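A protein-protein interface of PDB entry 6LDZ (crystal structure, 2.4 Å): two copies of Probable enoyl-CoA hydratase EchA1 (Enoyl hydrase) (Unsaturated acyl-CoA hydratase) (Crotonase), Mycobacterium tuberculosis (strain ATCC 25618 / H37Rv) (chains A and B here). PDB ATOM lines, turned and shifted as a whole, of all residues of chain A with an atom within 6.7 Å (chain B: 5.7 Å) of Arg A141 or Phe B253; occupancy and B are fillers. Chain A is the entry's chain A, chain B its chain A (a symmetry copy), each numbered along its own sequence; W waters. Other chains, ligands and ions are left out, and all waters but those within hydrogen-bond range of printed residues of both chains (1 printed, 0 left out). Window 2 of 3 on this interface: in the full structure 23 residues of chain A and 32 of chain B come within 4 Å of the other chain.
Of the 14 printed residues of chain B, 4 touch a printed residue of chain A. Printed residues of chain B that touch a printed residue of chain A: Ala B246, Gly B249, Phe B253 and Trp B261. Of the 8 printed residues of chain A, 4 touch a printed residue of chain B. Printed residues of chain A that touch a printed residue of chain B: Lys A140, Arg A141, Gly A142 and Leu A143. Hydrophobic or aromatic side chains of chain A within 4 Å of the printed part of chain B: Leu A143. Among the printed residues, no Asp or Glu carboxylate lies within 4 Å of a Lys or Arg side-chain nitrogen of the other chain.
Water W1 lies within hydrogen-bond range of the backbone carbonyl oxygen of Arg A141, the backbone carbonyl oxygen of Ala B246 and the backbone NH of Ala B250.
Of chain B, only Gly B249 (3.5 Å), Phe B253 (3.4 Å) and Trp B261 (3.7 Å) come within 4 Å of Arg A141. Phe B253 touches just these residues of chain A: Lys A140 (3.2 Å) and Arg A141 (3.4 Å). Printed residues of chain B within 4 Å of Gly A142: Trp B261. Of the printed residues of chain B, Lys A140 touches Phe B253 (3.2 Å) and Trp B261 (3.7 Å). Printed residues of chain B within 4 Å of Leu A143: Ala B246 (3.9 Å). Printed residues of chain A within 4 Å of Gly B249: Arg A141. Printed residues of chain A within 4 Å of Ala B246: Leu A143. Ala B254 touches none of the printed residues of chain A. Leu A77 touches none of the printed residues of chain B. The nearest residue of chain B that does not touch Arg A141 is Ala B246 (4.1 Å).
O of Glu A138 sits at hydrogen-bond distance from N of Leu A143 (3.1 Å).
Among the printed residues, pairs that only touch across the chains: Lys A140 with Phe B253 (3.2 Å), Lys A140 with Trp B261 (3.7 Å), Arg A141 with Gly B249 (3.5 Å), Arg A141 with Phe B253 (3.4 Å), Arg A141 with Trp B261 (3.7 Å), Gly A142 with Trp B261 (3.6 Å) and Leu A143 with Ala B246 (3.9 Å).
No position is printed for both chains. Of the 7 pairs that touch across the chains among the printed residues, none has its exchanged pair printed and touching as well.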
ATOM      1  N   LEU A  77      17.690 -21.286   7.984  1.00  0.00           N
ATOM      2  CA  LEU A  77      19.032 -21.835   8.144  1.00  0.00           C
ATOM      3  C   LEU A  77      19.132 -23.226   7.525  1.00  0.00           C
ATOM      4  O   LEU A  77      20.138 -23.553   6.883  1.00  0.00           O
ATOM      5  CB  LEU A  77      19.416 -21.859   9.620  1.00  0.00           C
ATOM      6  CG  LEU A  77      19.551 -20.480  10.287  1.00  0.00           C
ATOM      7  CD1 LEU A  77      20.145 -20.614  11.672  1.00  0.00           C
ATOM      8  CD2 LEU A  77      20.380 -19.527   9.441  1.00  0.00           C
ATOM      9  N   PRO A 137      21.112 -10.082  14.183  1.00  0.00           N
ATOM     10  CA  PRO A 137      22.112 -10.774  15.014  1.00  0.00           C
ATOM     11  C   PRO A 137      23.191 -11.544  14.247  1.00  0.00           C
ATOM     12  O   PRO A 137      23.878 -12.381  14.840  1.00  0.00           O
ATOM     13  CB  PRO A 137      21.248 -11.721  15.858  1.00  0.00           C
ATOM     14  CG  PRO A 137      20.071 -12.050  14.947  1.00  0.00           C
ATOM     15  CD  PRO A 137      19.849 -10.842  14.061  1.00  0.00           C
ATOM     16  N   GLU A 138      23.400 -11.241  12.964  1.00  0.00           N
ATOM     17  CA  GLU A 138      24.314 -12.042  12.146  1.00  0.00           C
ATOM     18  C   GLU A 138      25.710 -12.158  12.766  1.00  0.00           C
ATOM     19  O   GLU A 138      26.318 -13.236  12.735  1.00  0.00           O
ATOM     20  CB  GLU A 138      24.413 -11.455  10.733  1.00  0.00           C
ATOM     21  CG  GLU A 138      23.278 -11.894   9.778  1.00  0.00           C
ATOM     22  CD  GLU A 138      22.008 -11.044   9.913  1.00  0.00           C
ATOM     23  OE1 GLU A 138      21.831 -10.377  10.957  1.00  0.00           O
ATOM     24  OE2 GLU A 138      21.187 -11.029   8.961  1.00  0.00           O
ATOM     25  N   VAL A 139      26.240 -11.062  13.332  1.00  0.00           N
ATOM     26  CA  VAL A 139      27.610 -11.098  13.845  1.00  0.00           C
ATOM     27  C   VAL A 139      27.760 -12.115  14.973  1.00  0.00           C
ATOM     28  O   VAL A 139      28.852 -12.665  15.176  1.00  0.00           O
ATOM     29  CB  VAL A 139      28.078  -9.694  14.311  1.00  0.00           C
ATOM     30  CG1 VAL A 139      28.223  -8.735  13.115  1.00  0.00           C
ATOM     31  CG2 VAL A 139      27.131  -9.111  15.409  1.00  0.00           C
ATOM     32  N   LYS A 140      26.677 -12.395  15.707  1.00  0.00           N
ATOM     33  CA  LYS A 140      26.721 -13.405  16.755  1.00  0.00           C
ATOM     34  C   LYS A 140      27.087 -14.783  16.214  1.00  0.00           C
ATOM     35  O   LYS A 140      27.582 -15.617  16.975  1.00  0.00           O
ATOM     36  CB  LYS A 140      25.369 -13.481  17.470  1.00  0.00           C
ATOM     37  CG  LYS A 140      25.033 -12.288  18.358  1.00  0.00           C
ATOM     38  CD  LYS A 140      23.543 -12.267  18.595  1.00  0.00           C
ATOM     39  CE  LYS A 140      23.204 -12.176  20.058  1.00  0.00           C
ATOM     40  NZ  LYS A 140      22.796 -10.796  20.458  1.00  0.00           N
ATOM     41  N   ARG A 141      26.854 -15.043  14.926  1.00  0.00           N
ATOM     42  CA  ARG A 141      27.268 -16.287  14.291  1.00  0.00           C
ATOM     43  C   ARG A 141      28.536 -16.138  13.465  1.00  0.00           C
ATOM     44  O   ARG A 141      28.912 -17.079  12.749  1.00  0.00           O
ATOM     45  CB  ARG A 141      26.151 -16.835  13.408  1.00  0.00           C
ATOM     46  CG  ARG A 141      25.060 -17.472  14.200  1.00  0.00           C
ATOM     47  CD  ARG A 141      23.865 -17.776  13.323  1.00  0.00           C
ATOM     48  NE  ARG A 141      22.890 -18.564  14.059  1.00  0.00           N
ATOM     49  CZ  ARG A 141      22.719 -19.867  13.883  1.00  0.00           C
ATOM     50  NH1 ARG A 141      23.467 -20.503  12.990  1.00  0.00           N
ATOM     51  NH2 ARG A 141      21.810 -20.526  14.596  1.00  0.00           N
ATOM     52  N   GLY A 142      29.207 -14.995  13.546  1.00  0.00           N
ATOM     53  CA  GLY A 142      30.362 -14.788  12.693  1.00  0.00           C
ATOM     54  C   GLY A 142      30.010 -14.470  11.256  1.00  0.00           C
ATOM     55  O   GLY A 142      30.819 -14.715  10.354  1.00  0.00           O
ATOM     56  N   LEU A 143      28.820 -13.932  11.022  1.00  0.00           N
ATOM     57  CA  LEU A 143      28.343 -13.569   9.697  1.00  0.00           C
ATOM     58  C   LEU A 143      28.022 -12.075   9.666  1.00  0.00           C
ATOM     59  O   LEU A 143      28.158 -11.364  10.662  1.00  0.00           O
ATOM     60  CB  LEU A 143      27.124 -14.422   9.309  1.00  0.00           C
ATOM     61  CG  LEU A 143      27.416 -15.926   9.156  1.00  0.00           C
ATOM     62  CD1 LEU A 143      26.159 -16.734   8.785  1.00  0.00           C
ATOM     63  CD2 LEU A 143      28.539 -16.170   8.142  1.00  0.00           C
ATOM     64  N   ASP B 245      35.978 -18.658  11.153  1.00  0.00           N
ATOM     65  CA  ASP B 245      35.077 -18.260  12.234  1.00  0.00           C
ATOM     66  C   ASP B 245      33.624 -18.520  11.857  1.00  0.00           C
ATOM     67  O   ASP B 245      32.821 -18.952  12.701  1.00  0.00           O
ATOM     68  CB  ASP B 245      35.291 -16.785  12.580  1.00  0.00           C
ATOM     69  CG  ASP B 245      36.411 -16.569  13.598  1.00  0.00           C
ATOM     70  OD1 ASP B 245      36.952 -17.564  14.129  1.00  0.00           O
ATOM     71  OD2 ASP B 245      36.760 -15.393  13.853  1.00  0.00           O
ATOM     72  N   ALA B 246      33.276 -18.281  10.582  1.00  0.00           N
ATOM     73  CA  ALA B 246      31.928 -18.566  10.097  1.00  0.00           C
ATOM     74  C   ALA B 246      31.543 -20.030  10.321  1.00  0.00           C
ATOM     75  O   ALA B 246      30.428 -20.329  10.774  1.00  0.00           O
ATOM     76  CB  ALA B 246      31.823 -18.203   8.615  1.00  0.00           C
ATOM     77  N   GLU B 248      32.947 -22.001  12.575  1.00  0.00           N
ATOM     78  CA  GLU B 248      32.885 -22.183  14.022  1.00  0.00           C
ATOM     79  C   GLU B 248      31.589 -21.610  14.589  1.00  0.00           C
ATOM     80  O   GLU B 248      30.988 -22.189  15.506  1.00  0.00           O
ATOM     81  CB  GLU B 248      34.107 -21.540  14.688  1.00  0.00           C
ATOM     82  CG  GLU B 248      34.003 -21.372  16.204  1.00  0.00           C
ATOM     83  CD  GLU B 248      33.987 -22.706  16.943  1.00  0.00           C
ATOM     84  OE1 GLU B 248      34.235 -23.752  16.299  1.00  0.00           O
ATOM     85  OE2 GLU B 248      33.725 -22.705  18.170  1.00  0.00           O
ATOM     86  N   GLY B 249      31.135 -20.477  14.042  1.00  0.00           N
ATOM     87  CA  GLY B 249      29.868 -19.910  14.479  1.00  0.00           C
ATOM     88  C   GLY B 249      28.710 -20.870  14.287  1.00  0.00           C
ATOM     89  O   GLY B 249      27.877 -21.047  15.179  1.00  0.00           O
ATOM     90  N   ALA B 250      28.655 -21.522  13.127  1.00  0.00           N
ATOM     91  CA  ALA B 250      27.557 -22.448  12.859  1.00  0.00           C
ATOM     92  C   ALA B 250      27.631 -23.671  13.761  1.00  0.00           C
ATOM     93  O   ALA B 250      26.604 -24.130  14.275  1.00  0.00           O
ATOM     94  CB  ALA B 250      27.567 -22.873  11.389  1.00  0.00           C
ATOM     95  N   ILE B 251      28.830 -24.223  13.961  1.00  0.00           N
ATOM     96  CA  ILE B 251      28.960 -25.413  14.803  1.00  0.00           C
ATOM     97  C   ILE B 251      28.563 -25.095  16.240  1.00  0.00           C
ATOM     98  O   ILE B 251      27.870 -25.879  16.904  1.00  0.00           O
ATOM     99  CB  ILE B 251      30.391 -25.971  14.729  1.00  0.00           C
ATOM    100  CG1 ILE B 251      30.640 -26.611  13.365  1.00  0.00           C
ATOM    101  CG2 ILE B 251      30.636 -26.986  15.859  1.00  0.00           C
ATOM    102  CD1 ILE B 251      32.082 -26.930  13.120  1.00  0.00           C
ATOM    103  N   ALA B 252      28.998 -23.934  16.742  1.00  0.00           N
ATOM    104  CA  ALA B 252      28.756 -23.602  18.141  1.00  0.00           C
ATOM    105  C   ALA B 252      27.276 -23.352  18.402  1.00  0.00           C
ATOM    106  O   ALA B 252      26.740 -23.786  19.428  1.00  0.00           O
ATOM    107  CB  ALA B 252      29.601 -22.396  18.550  1.00  0.00           C
ATOM    108  N   PHE B 253      26.593 -22.675  17.480  1.00  0.00           N
ATOM    109  CA  PHE B 253      25.159 -22.477  17.653  1.00  0.00           C
ATOM    110  C   PHE B 253      24.416 -23.808  17.609  1.00  0.00           C
ATOM    111  O   PHE B 253      23.560 -24.072  18.461  1.00  0.00           O
ATOM    112  CB  PHE B 253      24.635 -21.501  16.599  1.00  0.00           C
ATOM    113  CG  PHE B 253      24.548 -20.088  17.093  1.00  0.00           C
ATOM    114  CD1 PHE B 253      23.340 -19.555  17.513  1.00  0.00           C
ATOM    115  CD2 PHE B 253      25.688 -19.297  17.176  1.00  0.00           C
ATOM    116  CE1 PHE B 253      23.267 -18.258  17.985  1.00  0.00           C
ATOM    117  CE2 PHE B 253      25.618 -17.999  17.648  1.00  0.00           C
ATOM    118  CZ  PHE B 253      24.407 -17.481  18.052  1.00  0.00           C
ATOM    119  N   ALA B 254      24.770 -24.679  16.653  1.00  0.00           N
ATOM    120  CA  ALA B 254      24.185 -26.017  16.594  1.00  0.00           C
ATOM    121  C   ALA B 254      24.371 -26.771  17.911  1.00  0.00           C
ATOM    122  O   ALA B 254      23.428 -27.389  18.419  1.00  0.00           O
ATOM    123  CB  ALA B 254      24.792 -26.804  15.430  1.00  0.00           C
ATOM    124  N   GLU B 255      25.575 -26.732  18.483  1.00  0.00           N
ATOM    125  CA  GLU B 255      25.833 -27.439  19.733  1.00  0.00           C
ATOM    126  C   GLU B 255      25.446 -26.614  20.972  1.00  0.00           C
ATOM    127  O   GLU B 255      25.722 -27.039  22.099  1.00  0.00           O
ATOM    128  CB  GLU B 255      27.311 -27.863  19.792  1.00  0.00           C
ATOM    129  CG  GLU B 255      27.729 -28.690  18.581  1.00  0.00           C
ATOM    130  CD  GLU B 255      29.167 -29.162  18.646  1.00  0.00           C
ATOM    131  OE1 GLU B 255      29.958 -28.571  19.414  1.00  0.00           O
ATOM    132  OE2 GLU B 255      29.515 -30.114  17.917  1.00  0.00           O
ATOM    133  N   ARG B 256      24.816 -25.449  20.784  1.00  0.00           N
ATOM    134  CA  ARG B 256      24.262 -24.653  21.886  1.00  0.00           C
ATOM    135  C   ARG B 256      25.336 -24.284  22.910  1.00  0.00           C
ATOM    136  O   ARG B 256      25.151 -24.407  24.121  1.00  0.00           O
ATOM    137  CB  ARG B 256      23.088 -25.386  22.539  1.00  0.00           C
ATOM    138  CG  ARG B 256      21.911 -25.545  21.584  1.00  0.00           C
ATOM    139  CD  ARG B 256      20.590 -25.762  22.304  1.00  0.00           C
ATOM    140  NE  ARG B 256      20.497 -27.091  22.890  1.00  0.00           N
ATOM    141  CZ  ARG B 256      19.765 -28.071  22.370  1.00  0.00           C
ATOM    142  NH1 ARG B 256      19.072 -27.857  21.253  1.00  0.00           N
ATOM    143  NH2 ARG B 256      19.723 -29.261  22.960  1.00  0.00           N
ATOM    144  N   ARG B 257      26.473 -23.814  22.403  1.00  0.00           N
ATOM    145  CA  ARG B 257      27.628 -23.479  23.218  1.00  0.00           C
ATOM    146  C   ARG B 257      28.283 -22.228  22.643  1.00  0.00           C
ATOM    147  O   ARG B 257      27.959 -21.775  21.540  1.00  0.00           O
ATOM    148  CB  ARG B 257      28.624 -24.645  23.271  1.00  0.00           C
ATOM    149  CG  ARG B 257      29.122 -25.102  21.899  1.00  0.00           C
ATOM    150  CD  ARG B 257      30.606 -25.430  21.911  1.00  0.00           C
ATOM    151  NE  ARG B 257      31.056 -26.005  20.642  1.00  0.00           N
ATOM    152  CZ  ARG B 257      31.877 -25.393  19.793  1.00  0.00           C
ATOM    153  NH1 ARG B 257      32.347 -24.182  20.075  1.00  0.00           N
ATOM    154  NH2 ARG B 257      32.227 -25.987  18.659  1.00  0.00           N
ATOM    155  N   PRO B 259      30.948 -19.863  20.878  1.00  0.00           N
ATOM    156  CA  PRO B 259      31.949 -20.062  19.830  1.00  0.00           C
ATOM    157  C   PRO B 259      33.301 -19.520  20.244  1.00  0.00           C
ATOM    158  O   PRO B 259      33.426 -18.540  20.987  1.00  0.00           O
ATOM    159  CB  PRO B 259      31.375 -19.293  18.634  1.00  0.00           C
ATOM    160  CG  PRO B 259      30.569 -18.237  19.245  1.00  0.00           C
ATOM    161  CD  PRO B 259      30.031 -18.751  20.565  1.00  0.00           C
ATOM    162  N   TRP B 261      36.337 -17.936  18.783  1.00  0.00           N
ATOM    163  CA  TRP B 261      36.800 -17.232  17.603  1.00  0.00           C
ATOM    164  C   TRP B 261      38.318 -17.289  17.527  1.00  0.00           C
ATOM    165  O   TRP B 261      39.018 -17.292  18.544  1.00  0.00           O
ATOM    166  CB  TRP B 261      36.328 -15.772  17.624  1.00  0.00           C
ATOM    167  CG  TRP B 261      34.854 -15.580  17.908  1.00  0.00           C
ATOM    168  CD1 TRP B 261      34.302 -14.923  18.980  1.00  0.00           C
ATOM    169  CD2 TRP B 261      33.752 -16.002  17.089  1.00  0.00           C
ATOM    170  NE1 TRP B 261      32.928 -14.937  18.889  1.00  0.00           N
ATOM    171  CE2 TRP B 261      32.567 -15.588  17.737  1.00  0.00           C
ATOM    172  CE3 TRP B 261      33.651 -16.704  15.886  1.00  0.00           C
ATOM    173  CZ2 TRP B 261      31.299 -15.850  17.219  1.00  0.00           C
ATOM    174  CZ3 TRP B 261      32.379 -16.970  15.371  1.00  0.00           C
ATOM    175  CH2 TRP B 261      31.222 -16.545  16.044  1.00  0.00           C
HETATM  176  O   HOH W   1      27.829 -18.943  11.039  1.00  0.00           O
